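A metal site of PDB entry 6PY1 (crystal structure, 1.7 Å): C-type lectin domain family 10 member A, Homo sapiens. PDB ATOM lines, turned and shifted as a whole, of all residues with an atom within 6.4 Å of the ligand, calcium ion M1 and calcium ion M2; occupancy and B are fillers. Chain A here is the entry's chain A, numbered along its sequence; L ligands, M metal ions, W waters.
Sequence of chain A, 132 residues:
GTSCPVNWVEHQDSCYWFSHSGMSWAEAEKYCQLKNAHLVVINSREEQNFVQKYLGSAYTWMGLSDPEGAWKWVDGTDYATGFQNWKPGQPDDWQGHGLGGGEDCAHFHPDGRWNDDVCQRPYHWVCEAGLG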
ATOM      1  N   TYR A  59      14.610 -25.466 -30.530  1.00  0.00           N
ATOM      2  CA  TYR A  59      15.514 -26.342 -29.763  1.00  0.00           C
ATOM      3  C   TYR A  59      14.738 -27.588 -29.370  1.00  0.00           C
ATOM      4  O   TYR A  59      13.618 -27.432 -28.899  1.00  0.00           O
ATOM      5  CB  TYR A  59      16.059 -25.632 -28.513  1.00  0.00           C
ATOM      6  CG  TYR A  59      16.983 -24.484 -28.795  1.00  0.00           C
ATOM      7  CD1 TYR A  59      17.723 -24.431 -29.944  1.00  0.00           C
ATOM      8  CD2 TYR A  59      17.019 -23.398 -27.943  1.00  0.00           C
ATOM      9  CE1 TYR A  59      18.527 -23.327 -30.233  1.00  0.00           C
ATOM     10  CE2 TYR A  59      17.822 -22.310 -28.198  1.00  0.00           C
ATOM     11  CZ  TYR A  59      18.606 -22.299 -29.327  1.00  0.00           C
ATOM     12  OH  TYR A  59      19.409 -21.210 -29.582  1.00  0.00           O
ATOM     13  N   ASP A  66      24.158 -36.380 -19.357  1.00  0.00           N
ATOM     14  CA  ASP A  66      25.396 -36.745 -18.612  1.00  0.00           C
ATOM     15  C   ASP A  66      25.330 -36.370 -17.139  1.00  0.00           C
ATOM     16  O   ASP A  66      26.357 -35.982 -16.595  1.00  0.00           O
ATOM     17  CB  ASP A  66      26.622 -36.140 -19.278  1.00  0.00           C
ATOM     18  CG  ASP A  66      26.844 -34.662 -19.003  1.00  0.00           C
ATOM     19  OD1 ASP A  66      25.839 -33.951 -18.742  1.00  0.00           O
ATOM     20  OD2 ASP A  66      28.018 -34.212 -19.002  1.00  0.00           O
ATOM     21  N   PRO A  67      24.200 -36.522 -16.427  1.00  0.00           N
ATOM     22  CA  PRO A  67      24.113 -36.001 -15.066  1.00  0.00           C
ATOM     23  C   PRO A  67      25.003 -36.784 -14.074  1.00  0.00           C
ATOM     24  O   PRO A  67      25.339 -36.218 -13.076  1.00  0.00           O
ATOM     25  CB  PRO A  67      22.629 -36.114 -14.724  1.00  0.00           C
ATOM     26  CG  PRO A  67      22.182 -37.303 -15.548  1.00  0.00           C
ATOM     27  CD  PRO A  67      22.961 -37.209 -16.839  1.00  0.00           C
ATOM     28  N   GLY A  69      28.130 -37.831 -14.790  1.00  0.00           N
ATOM     29  CA  GLY A  69      29.539 -37.680 -15.193  1.00  0.00           C
ATOM     30  C   GLY A  69      29.828 -37.937 -16.667  1.00  0.00           C
ATOM     31  O   GLY A  69      30.639 -37.184 -17.229  1.00  0.00           O
ATOM     32  N   TRP A  71      28.541 -38.918 -20.796  1.00  0.00           N
ATOM     33  CA  TRP A  71      27.416 -38.854 -21.791  1.00  0.00           C
ATOM     34  C   TRP A  71      26.881 -40.249 -22.049  1.00  0.00           C
ATOM     35  O   TRP A  71      27.681 -41.173 -22.342  1.00  0.00           O
ATOM     36  CB  TRP A  71      27.835 -38.160 -23.101  1.00  0.00           C
ATOM     37  CG  TRP A  71      28.001 -36.702 -22.879  1.00  0.00           C
ATOM     38  CD1 TRP A  71      29.130 -36.003 -22.634  1.00  0.00           C
ATOM     39  CD2 TRP A  71      26.906 -35.775 -22.787  1.00  0.00           C
ATOM     40  NE1 TRP A  71      28.829 -34.691 -22.420  1.00  0.00           N
ATOM     41  CE2 TRP A  71      27.473 -34.509 -22.523  1.00  0.00           C
ATOM     42  CE3 TRP A  71      25.515 -35.895 -22.897  1.00  0.00           C
ATOM     43  CZ2 TRP A  71      26.686 -33.380 -22.318  1.00  0.00           C
ATOM     44  CZ3 TRP A  71      24.729 -34.751 -22.726  1.00  0.00           C
ATOM     45  CH2 TRP A  71      25.325 -33.508 -22.461  1.00  0.00           C
ATOM     46  N   LYS A  87      27.678 -28.759 -31.849  1.00  0.00           N
ATOM     47  CA  LYS A  87      28.026 -27.368 -32.230  1.00  0.00           C
ATOM     48  C   LYS A  87      29.483 -27.116 -31.855  1.00  0.00           C
ATOM     49  O   LYS A  87      30.008 -27.705 -30.916  1.00  0.00           O
ATOM     50  CB  LYS A  87      27.165 -26.366 -31.460  1.00  0.00           C
ATOM     51  CG  LYS A  87      25.780 -26.133 -32.012  1.00  0.00           C
ATOM     52  CD  LYS A  87      25.776 -25.161 -33.189  1.00  0.00           C
ATOM     53  CE  LYS A  87      24.380 -24.746 -33.629  1.00  0.00           C
ATOM     54  NZ  LYS A  87      24.401 -24.032 -34.935  1.00  0.00           N
ATOM     55  N   GLY A  89      32.419 -25.730 -29.924  1.00  0.00           N
ATOM     56  CA  GLY A  89      32.586 -25.330 -28.520  1.00  0.00           C
ATOM     57  C   GLY A  89      31.753 -26.173 -27.565  1.00  0.00           C
ATOM     58  O   GLY A  89      31.913 -25.989 -26.369  1.00  0.00           O
ATOM     59  N   GLN A  90      30.888 -27.042 -28.074  1.00  0.00           N
ATOM     60  CA  GLN A  90      30.017 -27.903 -27.225  1.00  0.00           C
ATOM     61  C   GLN A  90      30.525 -29.341 -27.222  1.00  0.00           C
ATOM     62  O   GLN A  90      31.214 -29.783 -28.153  1.00  0.00           O
ATOM     63  CB  GLN A  90      28.581 -27.814 -27.752  1.00  0.00           C
ATOM     64  CG  GLN A  90      28.071 -26.387 -27.841  1.00  0.00           C
ATOM     65  CD  GLN A  90      28.041 -25.577 -26.555  1.00  0.00           C
ATOM     66  OE1 GLN A  90      27.993 -26.101 -25.470  1.00  0.00           O
ATOM     67  NE2 GLN A  90      27.909 -24.256 -26.670  1.00  0.00           N
ATOM     68  N   PRO A  91      30.218 -30.145 -26.184  1.00  0.00           N
ATOM     69  CA  PRO A  91      29.516 -29.700 -24.979  1.00  0.00           C
ATOM     70  C   PRO A  91      30.473 -28.930 -24.068  1.00  0.00           C
ATOM     71  O   PRO A  91      31.678 -29.209 -24.125  1.00  0.00           O
ATOM     72  CB  PRO A  91      29.107 -31.001 -24.305  1.00  0.00           C
ATOM     73  CG  PRO A  91      30.124 -32.010 -24.748  1.00  0.00           C
ATOM     74  CD  PRO A  91      30.567 -31.554 -26.113  1.00  0.00           C
ATOM     75  N   ASP A  92      29.955 -28.001 -23.259  1.00  0.00           N
ATOM     76  CA  ASP A  92      30.799 -27.140 -22.407  1.00  0.00           C
ATOM     77  C   ASP A  92      30.387 -27.212 -20.940  1.00  0.00           C
ATOM     78  O   ASP A  92      31.095 -26.595 -20.143  1.00  0.00           O
ATOM     79  CB  ASP A  92      30.831 -25.708 -22.925  1.00  0.00           C
ATOM     80  CG  ASP A  92      29.493 -25.006 -22.941  1.00  0.00           C
ATOM     81  OD1 ASP A  92      28.489 -25.703 -22.598  1.00  0.00           O
ATOM     82  OD2 ASP A  92      29.463 -23.809 -23.328  1.00  0.00           O
ATOM     83  N   ASP A  93      29.319 -27.932 -20.565  1.00  0.00           N
ATOM     84  CA  ASP A  93      28.860 -28.009 -19.166  1.00  0.00           C
ATOM     85  C   ASP A  93      28.789 -26.596 -18.563  1.00  0.00           C
ATOM     86  O   ASP A  93      29.220 -26.404 -17.384  1.00  0.00           O
ATOM     87  CB  ASP A  93      29.762 -28.915 -18.331  1.00  0.00           C
ATOM     88  CG  ASP A  93      29.128 -29.358 -17.011  1.00  0.00           C
ATOM     89  OD1 ASP A  93      27.935 -29.771 -17.013  1.00  0.00           O
ATOM     90  OD2 ASP A  93      29.841 -29.326 -15.982  1.00  0.00           O
ATOM     91  N   TRP A  94      28.311 -25.637 -19.340  1.00  0.00           N
ATOM     92  CA  TRP A  94      28.303 -24.201 -18.933  1.00  0.00           C
ATOM     93  C   TRP A  94      27.598 -24.009 -17.569  1.00  0.00           C
ATOM     94  O   TRP A  94      26.486 -24.528 -17.382  1.00  0.00           O
ATOM     95  CB  TRP A  94      27.653 -23.342 -19.968  1.00  0.00           C
ATOM     96  CG  TRP A  94      27.793 -21.876 -19.779  1.00  0.00           C
ATOM     97  CD1 TRP A  94      28.926 -21.135 -19.608  1.00  0.00           C
ATOM     98  CD2 TRP A  94      26.741 -20.938 -19.997  1.00  0.00           C
ATOM     99  NE1 TRP A  94      28.634 -19.801 -19.621  1.00  0.00           N
ATOM    100  CE2 TRP A  94      27.307 -19.651 -19.888  1.00  0.00           C
ATOM    101  CE3 TRP A  94      25.391 -21.062 -20.304  1.00  0.00           C
ATOM    102  CZ2 TRP A  94      26.531 -18.499 -20.002  1.00  0.00           C
ATOM    103  CZ3 TRP A  94      24.635 -19.926 -20.408  1.00  0.00           C
ATOM    104  CH2 TRP A  94      25.207 -18.660 -20.288  1.00  0.00           C
ATOM    105  N   GLY A 102      25.792 -27.272 -14.032  1.00  0.00           N
ATOM    106  CA  GLY A 102      26.283 -27.097 -15.395  1.00  0.00           C
ATOM    107  C   GLY A 102      25.176 -27.386 -16.385  1.00  0.00           C
ATOM    108  O   GLY A 102      24.090 -26.821 -16.231  1.00  0.00           O
ATOM    109  N   GLU A 103      25.432 -28.221 -17.374  1.00  0.00           N
ATOM    110  CA  GLU A 103      24.425 -28.490 -18.450  1.00  0.00           C
ATOM    111  C   GLU A 103      24.502 -29.984 -18.740  1.00  0.00           C
ATOM    112  O   GLU A 103      25.609 -30.480 -19.053  1.00  0.00           O
ATOM    113  CB  GLU A 103      24.683 -27.641 -19.699  1.00  0.00           C
ATOM    114  CG  GLU A 103      24.507 -26.140 -19.527  1.00  0.00           C
ATOM    115  CD  GLU A 103      24.855 -25.312 -20.738  1.00  0.00           C
ATOM    116  OE1 GLU A 103      24.071 -24.359 -21.108  1.00  0.00           O
ATOM    117  OE2 GLU A 103      25.899 -25.690 -21.368  1.00  0.00           O
ATOM    118  N   ASP A 104      23.423 -30.706 -18.535  1.00  0.00           N
ATOM    119  CA  ASP A 104      23.520 -32.186 -18.563  1.00  0.00           C
ATOM    120  C   ASP A 104      22.587 -32.839 -19.599  1.00  0.00           C
ATOM    121  O   ASP A 104      22.498 -34.085 -19.585  1.00  0.00           O
ATOM    122  CB  ASP A 104      23.264 -32.710 -17.150  1.00  0.00           C
ATOM    123  CG  ASP A 104      24.272 -32.256 -16.113  1.00  0.00           C
ATOM    124  OD1 ASP A 104      25.384 -31.805 -16.499  1.00  0.00           O
ATOM    125  OD2 ASP A 104      23.902 -32.302 -14.912  1.00  0.00           O
ATOM    126  N   CYS A 105      21.927 -32.108 -20.475  1.00  0.00           N
ATOM    127  CA  CYS A 105      20.966 -32.682 -21.451  1.00  0.00           C
ATOM    128  C   CYS A 105      21.255 -32.140 -22.857  1.00  0.00           C
ATOM    129  O   CYS A 105      21.423 -30.931 -22.969  1.00  0.00           O
ATOM    130  CB  CYS A 105      19.553 -32.330 -21.054  1.00  0.00           C
ATOM    131  SG  CYS A 105      18.989 -33.224 -19.587  1.00  0.00           S
ATOM    132  N   HIS A 107      20.403 -31.218 -26.823  1.00  0.00           N
ATOM    133  CA  HIS A 107      19.338 -30.850 -27.763  1.00  0.00           C
ATOM    134  C   HIS A 107      19.924 -30.500 -29.117  1.00  0.00           C
ATOM    135  O   HIS A 107      21.075 -30.038 -29.184  1.00  0.00           O
ATOM    136  CB  HIS A 107      18.452 -29.713 -27.205  1.00  0.00           C
ATOM    137  CG  HIS A 107      19.162 -28.399 -27.142  1.00  0.00           C
ATOM    138  ND1 HIS A 107      19.100 -27.496 -28.164  1.00  0.00           N
ATOM    139  CD2 HIS A 107      19.961 -27.858 -26.204  1.00  0.00           C
ATOM    140  CE1 HIS A 107      19.856 -26.431 -27.860  1.00  0.00           C
ATOM    141  NE2 HIS A 107      20.412 -26.633 -26.684  1.00  0.00           N
ATOM    142  N   HIS A 109      19.983 -27.823 -32.179  1.00  0.00           N
ATOM    143  CA  HIS A 109      19.641 -26.492 -32.758  1.00  0.00           C
ATOM    144  C   HIS A 109      18.856 -26.754 -34.040  1.00  0.00           C
ATOM    145  O   HIS A 109      18.906 -27.849 -34.622  1.00  0.00           O
ATOM    146  CB  HIS A 109      20.912 -25.741 -33.078  1.00  0.00           C
ATOM    147  CG  HIS A 109      21.530 -25.095 -31.898  1.00  0.00           C
ATOM    148  ND1 HIS A 109      21.628 -23.726 -31.780  1.00  0.00           N
ATOM    149  CD2 HIS A 109      22.047 -25.617 -30.766  1.00  0.00           C
ATOM    150  CE1 HIS A 109      22.221 -23.419 -30.640  1.00  0.00           C
ATOM    151  NE2 HIS A 109      22.503 -24.565 -30.000  1.00  0.00           N
ATOM    152  N   ASN A 115      23.820 -29.195 -28.676  1.00  0.00           N
ATOM    153  CA  ASN A 115      24.277 -28.390 -27.543  1.00  0.00           C
ATOM    154  C   ASN A 115      23.920 -29.125 -26.265  1.00  0.00           C
ATOM    155  O   ASN A 115      22.817 -29.699 -26.199  1.00  0.00           O
ATOM    156  CB  ASN A 115      23.746 -26.955 -27.580  1.00  0.00           C
ATOM    157  CG  ASN A 115      24.072 -26.206 -26.319  1.00  0.00           C
ATOM    158  OD1 ASN A 115      25.241 -26.108 -25.969  1.00  0.00           O
ATOM    159  ND2 ASN A 115      23.050 -25.730 -25.581  1.00  0.00           N
ATOM    160  N   ASP A 116      24.715 -28.944 -25.221  1.00  0.00           N
ATOM    161  CA  ASP A 116      24.315 -29.346 -23.855  1.00  0.00           C
ATOM    162  C   ASP A 116      23.654 -28.139 -23.167  1.00  0.00           C
ATOM    163  O   ASP A 116      24.160 -27.007 -23.219  1.00  0.00           O
ATOM    164  CB  ASP A 116      25.454 -29.960 -23.040  1.00  0.00           C
ATOM    165  CG  ASP A 116      26.659 -29.056 -22.831  1.00  0.00           C
ATOM    166  OD1 ASP A 116      26.886 -28.114 -23.654  1.00  0.00           O
ATOM    167  OD2 ASP A 116      27.334 -29.294 -21.826  1.00  0.00           O
ATOM    168  N   ASP A 117      22.544 -28.394 -22.504  1.00  0.00           N
ATOM    169  CA  ASP A 117      21.789 -27.280 -21.875  1.00  0.00           C
ATOM    170  C   ASP A 117      21.212 -27.769 -20.565  1.00  0.00           C
ATOM    171  O   ASP A 117      21.347 -28.953 -20.208  1.00  0.00           O
ATOM    172  CB  ASP A 117      20.718 -26.730 -22.860  1.00  0.00           C
ATOM    173  CG  ASP A 117      20.411 -25.220 -22.724  1.00  0.00           C
ATOM    174  OD1 ASP A 117      20.470 -24.712 -21.584  1.00  0.00           O
ATOM    175  OD2 ASP A 117      20.188 -24.527 -23.781  1.00  0.00           O
ATOM    176  N   VAL A 118      20.568 -26.847 -19.902  1.00  0.00           N
ATOM    177  CA  VAL A 118      19.932 -27.091 -18.589  1.00  0.00           C
ATOM    178  C   VAL A 118      18.702 -27.967 -18.822  1.00  0.00           C
ATOM    179  O   VAL A 118      17.788 -27.591 -19.568  1.00  0.00           O
ATOM    180  CB  VAL A 118      19.592 -25.753 -17.940  1.00  0.00           C
ATOM    181  CG1 VAL A 118      18.727 -25.968 -16.710  1.00  0.00           C
ATOM    182  CG2 VAL A 118      20.869 -24.968 -17.622  1.00  0.00           C
ATOM    183  N   TYR A 123      11.825 -27.550 -23.845  1.00  0.00           N
ATOM    184  CA  TYR A 123      12.146 -27.658 -25.264  1.00  0.00           C
ATOM    185  C   TYR A 123      11.207 -28.701 -25.898  1.00  0.00           C
ATOM    186  O   TYR A 123      10.547 -29.533 -25.201  1.00  0.00           O
ATOM    187  CB  TYR A 123      13.610 -28.057 -25.436  1.00  0.00           C
ATOM    188  CG  TYR A 123      14.643 -26.990 -25.172  1.00  0.00           C
ATOM    189  CD1 TYR A 123      14.332 -25.645 -25.075  1.00  0.00           C
ATOM    190  CD2 TYR A 123      15.980 -27.372 -25.037  1.00  0.00           C
ATOM    191  CE1 TYR A 123      15.322 -24.672 -24.910  1.00  0.00           C
ATOM    192  CE2 TYR A 123      16.961 -26.415 -24.859  1.00  0.00           C
ATOM    193  CZ  TYR A 123      16.632 -25.069 -24.803  1.00  0.00           C
ATOM    194  OH  TYR A 123      17.608 -24.139 -24.583  1.00  0.00           O
HETATM  195  O1  LIG L   1      26.531 -20.815 -25.241  1.00  0.00           O
HETATM  196  C1  LIG L   1      25.147 -20.962 -25.612  1.00  0.00           C
HETATM  197  O2  LIG L   1      24.279 -19.989 -24.965  1.00  0.00           O
HETATM  198  C2  LIG L   1      24.600 -22.372 -25.292  1.00  0.00           C
HETATM  199  N1  LIG L   1      23.171 -22.361 -25.614  1.00  0.00           N
HETATM  200  C3  LIG L   1      24.816 -22.762 -23.847  1.00  0.00           C
HETATM  201  O3  LIG L   1      24.550 -24.133 -23.593  1.00  0.00           O
HETATM  202  C4  LIG L   1      26.239 -22.491 -23.452  1.00  0.00           C
HETATM  203  O4  LIG L   1      26.976 -23.539 -24.059  1.00  0.00           O
HETATM  204  C5  LIG L   1      26.665 -21.037 -23.813  1.00  0.00           C
HETATM  205  C6  LIG L   1      28.106 -20.750 -23.411  1.00  0.00           C
HETATM  206  O5  LIG L   1      28.434 -19.381 -23.750  1.00  0.00           O
HETATM  207  C7  LIG L   1      22.716 -22.864 -26.795  1.00  0.00           C
HETATM  208  O6  LIG L   1      23.481 -23.323 -27.671  1.00  0.00           O
HETATM  209  C8  LIG L   1      21.215 -22.926 -26.960  1.00  0.00           C
HETATM  210 CA    CA M   1      26.277 -25.821 -23.759  1.00  0.00          CA
HETATM  211 CA    CA M   2      27.212 -31.877 -18.027  1.00  0.00          CA
HETATM  212  O   HOH W   1      25.614 -23.712 -29.147  1.00  0.00           O
HETATM  213  O   HOH W   2      21.091 -22.047 -23.530  1.00  0.00           O
HETATM  214  O   HOH W   3      27.759 -33.356 -15.947  1.00  0.00           O
HETATM  215  O   HOH W   4      29.686 -32.164 -17.597  1.00  0.00           O
HETATM  216  O   HOH W   5      28.167 -31.252 -20.094  1.00  0.00           O
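Within 4 Å of calcium ion M1: Gln 90, Asp 92, Glu 103, Asn 115 and Asp 116.
The nearest printed residue that does not touch calcium ion M2 is Trp 71 (4.6 Å).
Calcium ion M2 is bound by O of Glu 103, water W5, OD1 of Asp 104, OD1 of Asp 93, water W4, OD1 of Asp 66, water W3 and OD2 of Asp 66.
Calcium ion M2 has eight donor atoms within binding distance.
Water W1 lies within hydrogen-bond range of O6 of the ligand (2.6 Å), NE2 of His 109 (3.3 Å) and NE2 of Gln 90 (3.4 Å).
Water W2 lies within hydrogen-bond range of the side-chain carboxylate of Asp 117 (2.7 Å) and a nitrogen (N1) of the ligand (3.0 Å).
OE2 of Glu 103 lies close to N of Trp 94.
N of Asp 93 lies within hydrogen-bond range of OD2 of Asp 116 (2.7 Å).
The backbone NH (N) of Asp 104 is in hydrogen-bond range of the backbone carbonyl oxygen (O) of Asp 117 (3.2 Å).
The backbone NH (N) of Asn 115 is in hydrogen-bond range of the backbone carbonyl oxygen (O) of His 107 (2.9 Å).
The side-chain carboxylate (OD1) of Asp 92 sits close to the backbone NH (N) of Trp 94 (3.3 Å).
OD2 of Asp 117 sits at hydrogen-bond distance from OH of Tyr 123.
The backbone NH of Asp 117 sits at hydrogen-bond distance from the backbone carbonyl oxygen of Cys 105 (2.8 Å).
An oxygen (O6) of the ligand lies within hydrogen-bond range of a ring nitrogen (NE2) of His 109 (2.8 Å).
Calcium ion M1 is bound by the side-chain carboxylate (OD1) of Asp 116 (2.4 Å).
An oxygen (O4) of the ligand is bound to calcium ion M1 (2.4 Å).
An oxygen (O3) of the ligand is bound to calcium ion M1, at 2.4 Å.
Calcium ion M1 is bound by OE2 of Glu 103 (2.4 Å).
OE1 of Gln 90 is bound to calcium ion M1 (2.4 Å).
OD1 of Asn 115 is bound to calcium ion M1 (2.5 Å).
O of Asp 116 binds calcium ion M1, at 2.5 Å.
Calcium ion M1 is bound by the side-chain carboxylate (OD1) of Asp 92 (2.5 Å).
Merely in contact with the ligand: Trp 94 (3.6 Å), Tyr 59 (3.6 Å), Asp 117 (3.7 Å) and His 107 (3.8 Å).
Hydrophobic or aromatic side chains within 4 Å of the ligand: Tyr 59, Trp 94, His 107 and His 109.
The nearest printed residue that does not touch the ligand is Tyr 123 (4.5 Å).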
